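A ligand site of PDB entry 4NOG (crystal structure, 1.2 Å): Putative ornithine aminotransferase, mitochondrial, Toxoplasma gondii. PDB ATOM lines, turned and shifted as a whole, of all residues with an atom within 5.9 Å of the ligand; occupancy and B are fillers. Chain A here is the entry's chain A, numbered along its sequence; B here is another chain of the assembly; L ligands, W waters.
NE2 of Gln 245 is in hydrogen-bond range of O1 of the ligand, 3.0 Å away. An oxygen (O5) of the ligand is in hydrogen-bond range of the backbone NH (N) of Gly 121 (2.8 Å). The side-chain amino group (NZ) of Lys 271 lies within hydrogen-bond range of an oxygen (O2) of the ligand (2.7 Å). OD2 of Asp 242 is in hydrogen-bond range of N1 of the ligand (2.7 Å). The backbone NH of Thr 301 of chain B sits at hydrogen-bond distance from an oxygen (O4) of the ligand. An oxygen (O4) of the ligand lies within hydrogen-bond range of the side-chain hydroxyl (OG1) of Thr 301 of chain B. An oxygen (O6) of the ligand lies within hydrogen-bond range of the backbone NH (N) of Ala 122 (2.9 Å).
The side-chain hydroxyl (OH) of Tyr 156 is in hydrogen-bond range of the guanidinium group (NE) of Arg 159. N of Tyr 156 lies within hydrogen-bond range of OE2 of Glu 209 (3.2 Å). OG1 of Thr 120 is in hydrogen-bond range of OE2 of Glu 123 of chain B (2.9 Å). OE1 of Glu 209 sits at hydrogen-bond distance from N of Gly 213, at 3.0 Å. The side-chain hydroxyl of Thr 120 is in hydrogen-bond range of the backbone NH of Glu 123 of chain A (3.2 Å). NE2 of Gln 245 sits at hydrogen-bond distance from OE2 of Glu 214 (3.2 Å). N of Ile 244 sits at hydrogen-bond distance from OD1 of Asp 242. The side-chain amino group (NZ) of Lys 271 lies close to the backbone carbonyl oxygen (O) of Val 64, 3.2 Å away.
Residues that only touch the ligand: Trp 157 (3.4 Å), Tyr 156 (3.5 Å), Glu 209 (3.6 Å), Ile 244 (3.6 Å), Thr 120 (3.8 Å), Ser 300 of chain B (3.9 Å) and Gly 158 (3.97 Å). Hydrophobic or aromatic side chains within 4 Å of the ligand: Ala 122, Tyr 156 and Ile 244. 13 residues have an atom within 4 Å of the ligand: Thr 120, Gly 121, Ala 122, Tyr 156, Trp 157, Gly 158, Glu 209, Asp 242, Ile 244, Gln 245, Lys 271, Ser 300 of chain B and Thr 301 of chain B. The nearest printed residue that does not touch the ligand is Val 64 (4.04 Å).
Water W1 bridges the side-chain hydroxyl of Tyr 156 and an oxygen (O4) of the ligand. Water W8 lies within hydrogen-bond range of an oxygen (O5) of the ligand, the backbone NH (N) of Phe 302 of chain B, the side-chain hydroxyl (OG) of Ser 300 of chain B and the backbone NH (N) of Thr 301 of chain B. Water W3 lies within hydrogen-bond range of the side-chain hydroxyl of Ser 300 of chain B (2.7 Å), the side-chain carboxylate of Glu 123 of chain B (2.7 Å) and an oxygen (O6) of the ligand (2.8 Å). Water W5 lies within hydrogen-bond range of an oxygen (O6) of the ligand (2.9 Å) and the backbone NH of Arg 159 (3.1 Å). Water W6 lies within hydrogen-bond range of OE1 of Glu 209, N of Glu 214, O1 of the ligand and NE2 of Gln 245. Water W2 bridges OE1 of Glu 209 (2.7 Å) and N of Gly 213 (3.4 Å).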
ATOM      1  N   VAL A  64      -0.880 -17.928  11.445  1.00  0.00           N
ATOM      2  CA  VAL A  64      -0.340 -19.285  11.612  1.00  0.00           C
ATOM      3  C   VAL A  64       0.615 -19.637  10.489  1.00  0.00           C
ATOM      4  O   VAL A  64       0.521 -20.690   9.839  1.00  0.00           O
ATOM      5  CB  VAL A  64      -1.404 -20.374  11.906  1.00  0.00           C
ATOM      6  CG1 VAL A  64      -2.175 -20.007  13.177  1.00  0.00           C
ATOM      7  CG2 VAL A  64      -2.379 -20.600  10.759  1.00  0.00           C
ATOM      8  N   ASN A 119      -6.801 -22.039  -4.311  1.00  0.00           N
ATOM      9  CA  ASN A 119      -6.918 -20.797  -3.552  1.00  0.00           C
ATOM     10  C   ASN A 119      -6.613 -20.992  -2.076  1.00  0.00           C
ATOM     11  O   ASN A 119      -5.925 -20.204  -1.545  1.00  0.00           O
ATOM     12  CB  ASN A 119      -8.327 -20.203  -3.738  1.00  0.00           C
ATOM     13  CG  ASN A 119      -8.610 -20.050  -5.228  1.00  0.00           C
ATOM     14  OD1 ASN A 119      -8.162 -19.136  -5.854  1.00  0.00           O
ATOM     15  ND2 ASN A 119      -9.330 -21.011  -5.785  1.00  0.00           N
ATOM     16  N   THR A 120      -7.131 -22.021  -1.462  1.00  0.00           N
ATOM     17  CA  THR A 120      -6.973 -22.197  -0.019  1.00  0.00           C
ATOM     18  C   THR A 120      -6.243 -23.490   0.277  1.00  0.00           C
ATOM     19  O   THR A 120      -6.117 -24.372  -0.574  1.00  0.00           O
ATOM     20  CB  THR A 120      -8.335 -22.202   0.688  1.00  0.00           C
ATOM     21  OG1 THR A 120      -9.042 -23.380   0.310  1.00  0.00           O
ATOM     22  CG2 THR A 120      -9.136 -20.984   0.346  1.00  0.00           C
ATOM     23  N   GLY A 121      -5.788 -23.613   1.507  1.00  0.00           N
ATOM     24  CA  GLY A 121      -5.119 -24.866   1.889  1.00  0.00           C
ATOM     25  C   GLY A 121      -6.027 -26.055   1.839  1.00  0.00           C
ATOM     26  O   GLY A 121      -5.652 -27.112   1.371  1.00  0.00           O
ATOM     27  N   ALA A 122      -7.296 -25.859   2.282  1.00  0.00           N
ATOM     28  CA  ALA A 122      -8.251 -26.948   2.177  1.00  0.00           C
ATOM     29  C   ALA A 122      -8.422 -27.419   0.723  1.00  0.00           C
ATOM     30  O   ALA A 122      -8.544 -28.599   0.450  1.00  0.00           O
ATOM     31  CB  ALA A 122      -9.597 -26.487   2.714  1.00  0.00           C
ATOM     32  N   GLU A 123      -8.485 -26.460  -0.186  1.00  0.00           N
ATOM     33  CA  GLU A 123      -8.604 -26.832  -1.622  1.00  0.00           C
ATOM     34  C   GLU A 123      -7.376 -27.575  -2.141  1.00  0.00           C
ATOM     35  O   GLU A 123      -7.533 -28.464  -2.976  1.00  0.00           O
ATOM     36  CB  GLU A 123      -8.820 -25.587  -2.507  1.00  0.00           C
ATOM     37  CG  GLU A 123     -10.229 -25.000  -2.385  1.00  0.00           C
ATOM     38  CD  GLU A 123     -10.439 -23.941  -3.423  1.00  0.00           C
ATOM     39  OE1 GLU A 123      -9.487 -23.230  -3.850  1.00  0.00           O
ATOM     40  OE2 GLU A 123     -11.649 -23.767  -3.783  1.00  0.00           O
ATOM     41  N   TYR A 156      -4.654 -31.699  10.756  1.00  0.00           N
ATOM     42  CA  TYR A 156      -5.530 -30.611  10.325  1.00  0.00           C
ATOM     43  C   TYR A 156      -5.171 -30.261   8.924  1.00  0.00           C
ATOM     44  O   TYR A 156      -4.001 -29.990   8.602  1.00  0.00           O
ATOM     45  CB  TYR A 156      -5.359 -29.379  11.238  1.00  0.00           C
ATOM     46  CG  TYR A 156      -6.341 -28.302  10.857  1.00  0.00           C
ATOM     47  CD1 TYR A 156      -7.652 -28.294  11.390  1.00  0.00           C
ATOM     48  CD2 TYR A 156      -6.062 -27.296   9.992  1.00  0.00           C
ATOM     49  CE1 TYR A 156      -8.566 -27.318  11.054  1.00  0.00           C
ATOM     50  CE2 TYR A 156      -7.011 -26.327   9.666  1.00  0.00           C
ATOM     51  CZ  TYR A 156      -8.235 -26.335  10.212  1.00  0.00           C
ATOM     52  OH  TYR A 156      -9.177 -25.378   9.889  1.00  0.00           O
ATOM     53  N   TRP A 157      -6.163 -30.256   8.023  1.00  0.00           N
ATOM     54  CA  TRP A 157      -5.945 -29.815   6.660  1.00  0.00           C
ATOM     55  C   TRP A 157      -7.054 -28.952   6.138  1.00  0.00           C
ATOM     56  O   TRP A 157      -7.037 -28.561   4.960  1.00  0.00           O
ATOM     57  CB  TRP A 157      -5.617 -30.962   5.710  1.00  0.00           C
ATOM     58  CG  TRP A 157      -6.637 -32.006   5.500  1.00  0.00           C
ATOM     59  CD1 TRP A 157      -6.844 -33.173   6.239  1.00  0.00           C
ATOM     60  CD2 TRP A 157      -7.578 -32.075   4.410  1.00  0.00           C
ATOM     61  NE1 TRP A 157      -7.804 -33.942   5.679  1.00  0.00           N
ATOM     62  CE2 TRP A 157      -8.244 -33.298   4.516  1.00  0.00           C
ATOM     63  CE3 TRP A 157      -7.887 -31.209   3.344  1.00  0.00           C
ATOM     64  CZ2 TRP A 157      -9.255 -33.685   3.604  1.00  0.00           C
ATOM     65  CZ3 TRP A 157      -8.914 -31.579   2.469  1.00  0.00           C
ATOM     66  CH2 TRP A 157      -9.565 -32.794   2.575  1.00  0.00           C
ATOM     67  N   GLY A 158      -7.989 -28.543   6.978  1.00  0.00           N
ATOM     68  CA  GLY A 158      -9.054 -27.666   6.513  1.00  0.00           C
ATOM     69  C   GLY A 158     -10.410 -28.087   7.045  1.00  0.00           C
ATOM     70  O   GLY A 158     -10.537 -28.936   7.943  1.00  0.00           O
ATOM     71  N   ARG A 159     -11.430 -27.477   6.452  1.00  0.00           N
ATOM     72  CA  ARG A 159     -12.794 -27.482   6.982  1.00  0.00           C
ATOM     73  C   ARG A 159     -13.855 -27.934   5.995  1.00  0.00           C
ATOM     74  O   ARG A 159     -15.061 -27.857   6.331  1.00  0.00           O
ATOM     75  CB  ARG A 159     -13.138 -26.138   7.565  1.00  0.00           C
ATOM     76  CG  ARG A 159     -12.235 -25.692   8.692  1.00  0.00           C
ATOM     77  CD  ARG A 159     -12.525 -26.465   9.950  1.00  0.00           C
ATOM     78  NE  ARG A 159     -11.857 -25.840  11.077  1.00  0.00           N
ATOM     79  CZ  ARG A 159     -12.260 -25.927  12.315  1.00  0.00           C
ATOM     80  NH1 ARG A 159     -13.350 -26.601  12.669  1.00  0.00           N
ATOM     81  NH2 ARG A 159     -11.619 -25.266  13.234  1.00  0.00           N
ATOM     82  N   GLU A 209       1.772 -34.218   7.880  1.00  0.00           N
ATOM     83  CA  GLU A 209       2.412 -32.955   8.158  1.00  0.00           C
ATOM     84  C   GLU A 209       3.839 -33.260   8.703  1.00  0.00           C
ATOM     85  O   GLU A 209       3.963 -34.076   9.588  1.00  0.00           O
ATOM     86  CB  GLU A 209       1.637 -32.228   9.241  1.00  0.00           C
ATOM     87  CG  GLU A 209       0.221 -31.747   8.806  1.00  0.00           C
ATOM     88  CD  GLU A 209      -0.649 -31.306   9.999  1.00  0.00           C
ATOM     89  OE1 GLU A 209      -0.502 -30.122  10.446  1.00  0.00           O
ATOM     90  OE2 GLU A 209      -1.499 -32.098  10.442  1.00  0.00           O
ATOM     91  N   GLY A 213       0.674 -29.021  12.957  1.00  0.00           N
ATOM     92  CA  GLY A 213       0.491 -27.614  13.266  1.00  0.00           C
ATOM     93  C   GLY A 213      -0.579 -27.341  14.268  1.00  0.00           C
ATOM     94  O   GLY A 213      -0.310 -27.143  15.468  1.00  0.00           O
ATOM     95  N   GLU A 214      -1.812 -27.383  13.825  1.00  0.00           N
ATOM     96  CA  GLU A 214      -2.952 -27.213  14.708  1.00  0.00           C
ATOM     97  C   GLU A 214      -2.979 -28.271  15.795  1.00  0.00           C
ATOM     98  O   GLU A 214      -3.503 -28.014  16.868  1.00  0.00           O
ATOM     99  CB  GLU A 214      -4.229 -27.202  13.879  1.00  0.00           C
ATOM    100  CG  GLU A 214      -4.339 -26.047  12.874  1.00  0.00           C
ATOM    101  CD  GLU A 214      -4.062 -24.665  13.456  1.00  0.00           C
ATOM    102  OE1 GLU A 214      -4.923 -24.175  14.174  1.00  0.00           O
ATOM    103  OE2 GLU A 214      -2.978 -24.100  13.142  1.00  0.00           O
ATOM    104  N   ASP A 242       1.988 -32.202   3.560  1.00  0.00           N
ATOM    105  CA  ASP A 242       1.312 -30.905   3.715  1.00  0.00           C
ATOM    106  C   ASP A 242       2.319 -29.929   4.336  1.00  0.00           C
ATOM    107  O   ASP A 242       2.602 -30.024   5.554  1.00  0.00           O
ATOM    108  CB  ASP A 242       0.068 -31.056   4.566  1.00  0.00           C
ATOM    109  CG  ASP A 242      -0.718 -29.823   4.675  1.00  0.00           C
ATOM    110  OD1 ASP A 242      -0.197 -28.746   4.413  1.00  0.00           O
ATOM    111  OD2 ASP A 242      -1.925 -29.925   5.113  1.00  0.00           O
ATOM    112  N   GLU A 243       2.848 -29.010   3.538  1.00  0.00           N
ATOM    113  CA  GLU A 243       3.753 -27.968   3.963  1.00  0.00           C
ATOM    114  C   GLU A 243       3.073 -26.616   3.999  1.00  0.00           C
ATOM    115  O   GLU A 243       3.738 -25.561   3.976  1.00  0.00           O
ATOM    116  CB  GLU A 243       5.028 -27.962   3.099  1.00  0.00           C
ATOM    117  CG  GLU A 243       5.832 -29.235   3.294  1.00  0.00           C
ATOM    118  CD  GLU A 243       7.091 -29.055   4.100  1.00  0.00           C
ATOM    119  OE1 GLU A 243       7.285 -28.040   4.807  1.00  0.00           O
ATOM    120  OE2 GLU A 243       7.914 -30.002   4.001  1.00  0.00           O
ATOM    121  N   ILE A 244       1.723 -26.603   4.082  1.00  0.00           N
ATOM    122  CA  ILE A 244       0.975 -25.346   4.082  1.00  0.00           C
ATOM    123  C   ILE A 244       1.369 -24.488   5.301  1.00  0.00           C
ATOM    124  O   ILE A 244       1.485 -23.280   5.169  1.00  0.00           O
ATOM    125  CB  ILE A 244      -0.529 -25.621   4.017  1.00  0.00           C
ATOM    126  CG1 ILE A 244      -0.879 -26.171   2.627  1.00  0.00           C
ATOM    127  CG2 ILE A 244      -1.378 -24.378   4.382  1.00  0.00           C
ATOM    128  CD1 ILE A 244      -2.186 -26.937   2.554  1.00  0.00           C
ATOM    129  N   GLN A 245       1.580 -25.134   6.461  1.00  0.00           N
ATOM    130  CA  GLN A 245       2.018 -24.408   7.654  1.00  0.00           C
ATOM    131  C   GLN A 245       3.561 -24.460   7.894  1.00  0.00           C
ATOM    132  O   GLN A 245       4.124 -23.488   8.351  1.00  0.00           O
ATOM    133  CB  GLN A 245       1.286 -24.921   8.890  1.00  0.00           C
ATOM    134  CG  GLN A 245       1.590 -24.128  10.142  1.00  0.00           C
ATOM    135  CD  GLN A 245       0.782 -24.449  11.387  1.00  0.00           C
ATOM    136  OE1 GLN A 245       1.290 -24.295  12.496  1.00  0.00           O
ATOM    137  NE2 GLN A 245      -0.463 -24.805  11.241  1.00  0.00           N
ATOM    138  N   THR A 246       4.185 -25.601   7.567  1.00  0.00           N
ATOM    139  CA  THR A 246       5.580 -25.789   7.874  1.00  0.00           C
ATOM    140  C   THR A 246       6.533 -25.334   6.805  1.00  0.00           C
ATOM    141  O   THR A 246       7.743 -25.263   7.067  1.00  0.00           O
ATOM    142  CB  THR A 246       5.841 -27.259   8.179  1.00  0.00           C
ATOM    143  OG1 THR A 246       5.520 -28.067   7.057  1.00  0.00           O
ATOM    144  CG2 THR A 246       5.108 -27.733   9.381  1.00  0.00           C
ATOM    145  N   LYS A 271      -0.754 -20.514   2.554  1.00  0.00           N
ATOM    146  CA  LYS A 271      -0.392 -19.539   3.572  1.00  0.00           C
ATOM    147  C   LYS A 271       0.651 -18.511   3.095  1.00  0.00           C
ATOM    148  O   LYS A 271       0.288 -17.613   2.319  1.00  0.00           O
ATOM    149  CB  LYS A 271      -0.101 -20.247   4.888  1.00  0.00           C
ATOM    150  CG  LYS A 271      -1.349 -20.843   5.536  1.00  0.00           C
ATOM    151  CD  LYS A 271      -1.065 -21.402   6.899  1.00  0.00           C
ATOM    152  CE  LYS A 271      -2.279 -21.914   7.608  1.00  0.00           C
ATOM    153  NZ  LYS A 271      -1.849 -22.550   8.885  1.00  0.00           N
ATOM    154  N   GLU B 123     -16.088 -23.438  -1.300  1.00  0.00           N
ATOM    155  CA  GLU B 123     -16.074 -23.347   0.159  1.00  0.00           C
ATOM    156  C   GLU B 123     -17.386 -22.826   0.671  1.00  0.00           C
ATOM    157  O   GLU B 123     -17.775 -23.221   1.784  1.00  0.00           O
ATOM    158  CB  GLU B 123     -14.940 -22.451   0.631  1.00  0.00           C
ATOM    159  CG  GLU B 123     -13.559 -23.057   0.523  1.00  0.00           C
ATOM    160  CD  GLU B 123     -12.498 -22.194   1.167  1.00  0.00           C
ATOM    161  OE1 GLU B 123     -12.670 -20.934   1.223  1.00  0.00           O
ATOM    162  OE2 GLU B 123     -11.510 -22.806   1.638  1.00  0.00           O
ATOM    163  N   GLY B 299     -13.927 -22.853  10.220  1.00  0.00           N
ATOM    164  CA  GLY B 299     -12.833 -21.888  10.170  1.00  0.00           C
ATOM    165  C   GLY B 299     -12.292 -21.805   8.732  1.00  0.00           C
ATOM    166  O   GLY B 299     -12.740 -22.545   7.869  1.00  0.00           O
ATOM    167  N   SER B 300     -11.356 -20.891   8.567  1.00  0.00           N
ATOM    168  CA  SER B 300     -10.616 -20.735   7.274  1.00  0.00           C
ATOM    169  C   SER B 300      -9.527 -19.721   7.540  1.00  0.00           C
ATOM    170  O   SER B 300      -9.790 -18.674   8.144  1.00  0.00           O
ATOM    171  CB  SER B 300     -11.551 -20.131   6.247  1.00  0.00           C
ATOM    172  OG  SER B 300     -10.904 -19.715   5.124  1.00  0.00           O
ATOM    173  N   THR B 301      -8.318 -19.977   7.023  1.00  0.00           N
ATOM    174  CA  THR B 301      -7.250 -19.024   7.195  1.00  0.00           C
ATOM    175  C   THR B 301      -7.588 -17.658   6.661  1.00  0.00           C
ATOM    176  O   THR B 301      -7.507 -16.639   7.363  1.00  0.00           O
ATOM    177  CB  THR B 301      -5.956 -19.548   6.619  1.00  0.00           C
ATOM    178  OG1 THR B 301      -5.607 -20.749   7.283  1.00  0.00           O
ATOM    179  CG2 THR B 301      -4.812 -18.541   6.808  1.00  0.00           C
ATOM    180  N   PHE B 302      -7.909 -17.627   5.373  1.00  0.00           N
ATOM    181  CA  PHE B 302      -8.130 -16.357   4.680  1.00  0.00           C
ATOM    182  C   PHE B 302      -9.570 -15.849   4.697  1.00  0.00           C
ATOM    183  O   PHE B 302      -9.824 -14.748   4.267  1.00  0.00           O
ATOM    184  CB  PHE B 302      -7.604 -16.406   3.210  1.00  0.00           C
ATOM    185  CG  PHE B 302      -6.096 -16.359   3.098  1.00  0.00           C
ATOM    186  CD1 PHE B 302      -5.333 -17.510   3.182  1.00  0.00           C
ATOM    187  CD2 PHE B 302      -5.464 -15.159   2.947  1.00  0.00           C
ATOM    188  CE1 PHE B 302      -3.956 -17.488   3.053  1.00  0.00           C
ATOM    189  CE2 PHE B 302      -4.083 -15.132   2.826  1.00  0.00           C
ATOM    190  CZ  PHE B 302      -3.350 -16.289   2.891  1.00  0.00           C
HETATM  191  N1  LIG L   1      -2.981 -27.630   6.113  1.00  0.00           N
HETATM  192  C1  LIG L   1      -2.385 -27.186   7.203  1.00  0.00           C
HETATM  193  C2  LIG L   1      -1.163 -27.856   7.721  1.00  0.00           C
HETATM  194  C3  LIG L   1      -2.907 -26.023   7.868  1.00  0.00           C
HETATM  195  O1  LIG L   1      -2.315 -25.633   9.041  1.00  0.00           O
HETATM  196  C4  LIG L   1      -4.088 -25.368   7.362  1.00  0.00           C
HETATM  197  C5  LIG L   1      -4.652 -24.188   8.052  1.00  0.00           C
HETATM  198  O2  LIG L   1      -4.240 -23.805   9.161  1.00  0.00           O
HETATM  199  C6  LIG L   1      -4.693 -25.954   6.192  1.00  0.00           C
HETATM  200  C7  LIG L   1      -4.105 -27.069   5.604  1.00  0.00           C
HETATM  201  C8  LIG L   1      -5.935 -25.359   5.650  1.00  0.00           C
HETATM  202  O3  LIG L   1      -5.644 -24.102   5.018  1.00  0.00           O
HETATM  203  P1  LIG L   1      -6.842 -23.035   4.784  1.00  0.00           P
HETATM  204  O4  LIG L   1      -7.207 -22.484   6.138  1.00  0.00           O
HETATM  205  O5  LIG L   1      -6.208 -22.033   3.807  1.00  0.00           O
HETATM  206  O6  LIG L   1      -7.998 -23.784   4.139  1.00  0.00           O
HETATM  207  O   HOH W   1      -8.723 -23.478   8.139  1.00  0.00           O
HETATM  208  O   HOH W   2       1.592 -28.516   9.766  1.00  0.00           O
HETATM  209  O   HOH W   3      -9.995 -21.841   3.703  1.00  0.00           O
HETATM  210  O   HOH W   4      -3.487 -21.426   2.769  1.00  0.00           O
HETATM  211  O   HOH W   5     -10.213 -24.664   5.755  1.00  0.00           O
HETATM  212  O   HOH W   6      -2.123 -27.867  10.987  1.00  0.00           O
HETATM  213  O   HOH W   7       2.276 -27.834   7.209  1.00  0.00           O
HETATM  214  O   HOH W   8      -7.890 -19.869   3.558  1.00  0.00           O
